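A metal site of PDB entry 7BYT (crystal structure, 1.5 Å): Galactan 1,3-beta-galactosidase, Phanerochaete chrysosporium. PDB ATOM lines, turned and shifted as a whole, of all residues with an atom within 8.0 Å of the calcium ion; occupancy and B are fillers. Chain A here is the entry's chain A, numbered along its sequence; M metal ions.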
ATOM      1  N   TYR A 307      31.147  17.653 -19.654  1.00  0.00           N
ATOM      2  CA  TYR A 307      31.476  18.495 -20.796  1.00  0.00           C
ATOM      3  C   TYR A 307      30.393  18.292 -21.835  1.00  0.00           C
ATOM      4  O   TYR A 307      30.153  17.159 -22.267  1.00  0.00           O
ATOM      5  CB  TYR A 307      32.825  18.093 -21.402  1.00  0.00           C
ATOM      6  CG  TYR A 307      33.993  18.204 -20.441  1.00  0.00           C
ATOM      7  CD1 TYR A 307      34.301  17.166 -19.562  1.00  0.00           C
ATOM      8  CD2 TYR A 307      34.773  19.359 -20.397  1.00  0.00           C
ATOM      9  CE1 TYR A 307      35.354  17.279 -18.664  1.00  0.00           C
ATOM     10  CE2 TYR A 307      35.836  19.466 -19.511  1.00  0.00           C
ATOM     11  CZ  TYR A 307      36.119  18.424 -18.647  1.00  0.00           C
ATOM     12  OH  TYR A 307      37.166  18.527 -17.765  1.00  0.00           O
ATOM     13  N   GLU A 308      29.734  19.370 -22.242  1.00  0.00           N
ATOM     14  CA  GLU A 308      28.667  19.262 -23.238  1.00  0.00           C
ATOM     15  C   GLU A 308      29.263  19.085 -24.616  1.00  0.00           C
ATOM     16  O   GLU A 308      30.205  19.784 -24.995  1.00  0.00           O
ATOM     17  CB  GLU A 308      27.790  20.516 -23.231  1.00  0.00           C
ATOM     18  CG  GLU A 308      27.084  20.794 -21.934  1.00  0.00           C
ATOM     19  CD  GLU A 308      25.936  19.831 -21.649  1.00  0.00           C
ATOM     20  OE1 GLU A 308      25.579  18.991 -22.519  1.00  0.00           O
ATOM     21  OE2 GLU A 308      25.365  19.938 -20.544  1.00  0.00           O
ATOM     22  N   ALA A 309      28.734  18.138 -25.385  1.00  0.00           N
ATOM     23  CA  ALA A 309      29.265  17.905 -26.729  1.00  0.00           C
ATOM     24  C   ALA A 309      29.084  19.129 -27.622  1.00  0.00           C
ATOM     25  O   ALA A 309      29.950  19.441 -28.454  1.00  0.00           O
ATOM     26  CB  ALA A 309      28.619  16.672 -27.347  1.00  0.00           C
ATOM     27  N   GLU A 310      27.954  19.832 -27.469  1.00  0.00           N
ATOM     28  CA  GLU A 310      27.630  20.995 -28.288  1.00  0.00           C
ATOM     29  C   GLU A 310      28.574  22.167 -28.024  1.00  0.00           C
ATOM     30  O   GLU A 310      28.601  23.106 -28.835  1.00  0.00           O
ATOM     31  CB  GLU A 310      26.176  21.414 -28.055  1.00  0.00           C
ATOM     32  CG  GLU A 310      25.846  21.820 -26.628  1.00  0.00           C
ATOM     33  CD  GLU A 310      25.322  20.664 -25.775  1.00  0.00           C
ATOM     34  OE1 GLU A 310      25.685  19.497 -26.045  1.00  0.00           O
ATOM     35  OE2 GLU A 310      24.525  20.928 -24.848  1.00  0.00           O
ATOM     36  N   ASN A 311      29.340  22.134 -26.937  1.00  0.00           N
ATOM     37  CA  ASN A 311      30.354  23.153 -26.670  1.00  0.00           C
ATOM     38  C   ASN A 311      31.707  22.790 -27.266  1.00  0.00           C
ATOM     39  O   ASN A 311      32.639  23.590 -27.200  1.00  0.00           O
ATOM     40  CB  ASN A 311      30.493  23.418 -25.167  1.00  0.00           C
ATOM     41  CG  ASN A 311      29.266  24.111 -24.580  1.00  0.00           C
ATOM     42  OD1 ASN A 311      28.521  24.779 -25.297  1.00  0.00           O
ATOM     43  ND2 ASN A 311      29.058  23.944 -23.275  1.00  0.00           N
ATOM     44  N   LEU A 321      21.851  19.391 -32.625  1.00  0.00           N
ATOM     45  CA  LEU A 321      20.469  18.975 -32.413  1.00  0.00           C
ATOM     46  C   LEU A 321      19.929  19.641 -31.163  1.00  0.00           C
ATOM     47  O   LEU A 321      20.662  19.846 -30.185  1.00  0.00           O
ATOM     48  CB  LEU A 321      20.395  17.457 -32.187  1.00  0.00           C
ATOM     49  CG  LEU A 321      20.958  16.569 -33.286  1.00  0.00           C
ATOM     50  CD1 LEU A 321      20.868  15.091 -32.895  1.00  0.00           C
ATOM     51  CD2 LEU A 321      20.192  16.825 -34.568  1.00  0.00           C
ATOM     52  N   GLY A 323      16.860  19.295 -28.234  1.00  0.00           N
ATOM     53  CA  GLY A 323      15.888  18.381 -27.667  1.00  0.00           C
ATOM     54  C   GLY A 323      15.799  18.459 -26.166  1.00  0.00           C
ATOM     55  O   GLY A 323      16.813  18.665 -25.477  1.00  0.00           O
ATOM     56  N   GLY A 325      15.366  16.161 -24.097  1.00  0.00           N
ATOM     57  CA  GLY A 325      15.964  15.049 -23.401  1.00  0.00           C
ATOM     58  C   GLY A 325      17.450  15.169 -23.193  1.00  0.00           C
ATOM     59  O   GLY A 325      18.036  14.302 -22.541  1.00  0.00           O
ATOM     60  N   PHE A 326      18.058  16.220 -23.731  1.00  0.00           N
ATOM     61  CA  PHE A 326      19.498  16.419 -23.684  1.00  0.00           C
ATOM     62  C   PHE A 326      19.859  17.375 -22.569  1.00  0.00           C
ATOM     63  O   PHE A 326      19.162  18.362 -22.334  1.00  0.00           O
ATOM     64  CB  PHE A 326      20.011  17.047 -24.980  1.00  0.00           C
ATOM     65  CG  PHE A 326      19.662  16.281 -26.223  1.00  0.00           C
ATOM     66  CD1 PHE A 326      19.839  14.900 -26.304  1.00  0.00           C
ATOM     67  CD2 PHE A 326      19.215  16.955 -27.351  1.00  0.00           C
ATOM     68  CE1 PHE A 326      19.536  14.210 -27.476  1.00  0.00           C
ATOM     69  CE2 PHE A 326      18.921  16.277 -28.520  1.00  0.00           C
ATOM     70  CZ  PHE A 326      19.073  14.902 -28.585  1.00  0.00           C
ATOM     71  N   SER A 327      20.988  17.103 -21.914  1.00  0.00           N
ATOM     72  CA  SER A 327      21.638  18.117 -21.092  1.00  0.00           C
ATOM     73  C   SER A 327      21.907  19.375 -21.892  1.00  0.00           C
ATOM     74  O   SER A 327      22.420  19.318 -23.024  1.00  0.00           O
ATOM     75  CB  SER A 327      22.966  17.581 -20.538  1.00  0.00           C
ATOM     76  OG  SER A 327      23.460  18.449 -19.533  1.00  0.00           O
ATOM     77  N   GLY A 328      21.569  20.521 -21.320  1.00  0.00           N
ATOM     78  CA  GLY A 328      21.712  21.769 -22.048  1.00  0.00           C
ATOM     79  C   GLY A 328      20.736  21.947 -23.187  1.00  0.00           C
ATOM     80  O   GLY A 328      20.824  22.954 -23.900  1.00  0.00           O
ATOM     81  N   GLY A 329      19.795  21.025 -23.368  1.00  0.00           N
ATOM     82  CA  GLY A 329      18.862  21.072 -24.472  1.00  0.00           C
ATOM     83  C   GLY A 329      19.468  20.814 -25.837  1.00  0.00           C
ATOM     84  O   GLY A 329      18.784  21.001 -26.841  1.00  0.00           O
ATOM     85  N   LYS A 330      20.737  20.418 -25.902  1.00  0.00           N
ATOM     86  CA  LYS A 330      21.414  20.268 -27.187  1.00  0.00           C
ATOM     87  C   LYS A 330      22.302  19.031 -27.183  1.00  0.00           C
ATOM     88  O   LYS A 330      22.745  18.557 -26.137  1.00  0.00           O
ATOM     89  CB  LYS A 330      22.233  21.515 -27.539  1.00  0.00           C
ATOM     90  CG  LYS A 330      21.383  22.771 -27.715  1.00  0.00           C
ATOM     91  CD  LYS A 330      22.233  23.941 -28.200  1.00  0.00           C
ATOM     92  CE  LYS A 330      21.373  25.171 -28.430  1.00  0.00           C
ATOM     93  NZ  LYS A 330      19.953  24.827 -28.762  1.00  0.00           N
ATOM     94  N   ALA A 331      22.569  18.537 -28.396  1.00  0.00           N
ATOM     95  CA  ALA A 331      23.459  17.408 -28.612  1.00  0.00           C
ATOM     96  C   ALA A 331      24.102  17.616 -29.973  1.00  0.00           C
ATOM     97  O   ALA A 331      23.720  18.496 -30.736  1.00  0.00           O
ATOM     98  CB  ALA A 331      22.697  16.070 -28.578  1.00  0.00           C
ATOM     99  N   VAL A 332      25.099  16.788 -30.285  1.00  0.00           N
ATOM    100  CA  VAL A 332      25.745  16.820 -31.593  1.00  0.00           C
ATOM    101  C   VAL A 332      25.244  15.641 -32.392  1.00  0.00           C
ATOM    102  O   VAL A 332      25.345  14.493 -31.945  1.00  0.00           O
ATOM    103  CB  VAL A 332      27.275  16.826 -31.473  1.00  0.00           C
ATOM    104  CG1 VAL A 332      27.923  16.758 -32.864  1.00  0.00           C
ATOM    105  CG2 VAL A 332      27.744  18.078 -30.736  1.00  0.00           C
ATOM    106  N   TYR A 358      27.184  10.145 -22.839  1.00  0.00           N
ATOM    107  CA  TYR A 358      25.733  10.295 -22.789  1.00  0.00           C
ATOM    108  C   TYR A 358      25.251  10.562 -24.208  1.00  0.00           C
ATOM    109  O   TYR A 358      25.687  11.521 -24.842  1.00  0.00           O
ATOM    110  CB  TYR A 358      25.366  11.460 -21.874  1.00  0.00           C
ATOM    111  CG  TYR A 358      25.423  11.083 -20.406  1.00  0.00           C
ATOM    112  CD1 TYR A 358      26.637  10.809 -19.789  1.00  0.00           C
ATOM    113  CD2 TYR A 358      24.253  10.951 -19.668  1.00  0.00           C
ATOM    114  CE1 TYR A 358      26.683  10.432 -18.455  1.00  0.00           C
ATOM    115  CE2 TYR A 358      24.294  10.585 -18.327  1.00  0.00           C
ATOM    116  CZ  TYR A 358      25.520  10.318 -17.743  1.00  0.00           C
ATOM    117  OH  TYR A 358      25.540   9.938 -16.422  1.00  0.00           O
ATOM    118  N   VAL A 392      18.216   9.820 -23.613  1.00  0.00           N
ATOM    119  CA  VAL A 392      19.658   9.693 -23.402  1.00  0.00           C
ATOM    120  C   VAL A 392      19.945   8.603 -22.371  1.00  0.00           C
ATOM    121  O   VAL A 392      19.329   8.563 -21.303  1.00  0.00           O
ATOM    122  CB  VAL A 392      20.253  11.045 -22.945  1.00  0.00           C
ATOM    123  CG1 VAL A 392      21.712  10.884 -22.506  1.00  0.00           C
ATOM    124  CG2 VAL A 392      20.132  12.058 -24.077  1.00  0.00           C
ATOM    125  N   LEU A 421      25.577  12.663 -29.630  1.00  0.00           N
ATOM    126  CA  LEU A 421      26.336  12.808 -28.386  1.00  0.00           C
ATOM    127  C   LEU A 421      25.831  14.021 -27.618  1.00  0.00           C
ATOM    128  O   LEU A 421      25.900  15.158 -28.113  1.00  0.00           O
ATOM    129  CB  LEU A 421      27.830  12.952 -28.691  1.00  0.00           C
ATOM    130  CG  LEU A 421      28.744  12.831 -27.471  1.00  0.00           C
ATOM    131  CD1 LEU A 421      28.627  11.478 -26.769  1.00  0.00           C
ATOM    132  CD2 LEU A 421      30.193  13.115 -27.891  1.00  0.00           C
ATOM    133  N   ASP A 422      25.349  13.784 -26.402  1.00  0.00           N
ATOM    134  CA  ASP A 422      24.810  14.845 -25.560  1.00  0.00           C
ATOM    135  C   ASP A 422      25.910  15.510 -24.755  1.00  0.00           C
ATOM    136  O   ASP A 422      26.078  16.742 -24.787  1.00  0.00           O
ATOM    137  CB  ASP A 422      23.752  14.219 -24.647  1.00  0.00           C
ATOM    138  CG  ASP A 422      23.129  15.209 -23.682  1.00  0.00           C
ATOM    139  OD1 ASP A 422      23.370  16.425 -23.814  1.00  0.00           O
ATOM    140  OD2 ASP A 422      22.380  14.750 -22.791  1.00  0.00           O
ATOM    141  N   LYS A 423      26.675  14.707 -24.030  1.00  0.00           N
ATOM    142  CA  LYS A 423      27.743  15.203 -23.165  1.00  0.00           C
ATOM    143  C   LYS A 423      28.588  13.991 -22.792  1.00  0.00           C
ATOM    144  O   LYS A 423      28.221  12.840 -23.058  1.00  0.00           O
ATOM    145  CB  LYS A 423      27.169  15.877 -21.909  1.00  0.00           C
ATOM    146  CG  LYS A 423      26.447  14.926 -20.928  1.00  0.00           C
ATOM    147  CD  LYS A 423      26.198  15.658 -19.630  1.00  0.00           C
ATOM    148  CE  LYS A 423      25.757  14.752 -18.509  1.00  0.00           C
ATOM    149  NZ  LYS A 423      25.923  15.524 -17.236  1.00  0.00           N
ATOM    150  N   ILE A 424      29.711  14.275 -22.140  1.00  0.00           N
ATOM    151  CA  ILE A 424      30.511  13.237 -21.495  1.00  0.00           C
ATOM    152  C   ILE A 424      30.712  13.646 -20.045  1.00  0.00           C
ATOM    153  O   ILE A 424      30.636  14.819 -19.687  1.00  0.00           O
ATOM    154  CB  ILE A 424      31.857  12.984 -22.199  1.00  0.00           C
ATOM    155  CG1 ILE A 424      32.796  14.189 -22.029  1.00  0.00           C
ATOM    156  CG2 ILE A 424      31.619  12.682 -23.683  1.00  0.00           C
ATOM    157  CD1 ILE A 424      34.201  13.928 -22.610  1.00  0.00           C
HETATM  158 CA    CA M   1      24.259  18.475 -24.330  1.00  0.00          CA
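O of Tyr 358 lies within hydrogen-bond range of N of Asp 422 (2.8 Å).
The backbone carbonyl oxygen (O) of Asp 422 sits close to the backbone NH (N) of Ala 309 (3.1 Å).
The calcium ion is bound by OD1 of Asp 422 (2.3 Å), OE1 of Glu 308 (2.3 Å), O of Lys 330 (2.4 Å), O of Ser 327 (2.4 Å), OE1 of Glu 310 (2.5 Å), OE2 of Glu 310 (2.5 Å) and O of Asp 422 (2.6 Å).
Five residues have an atom within 4 Å of the calcium ion: Glu 308, Glu 310, Ser 327, Lys 330 and Asp 422.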
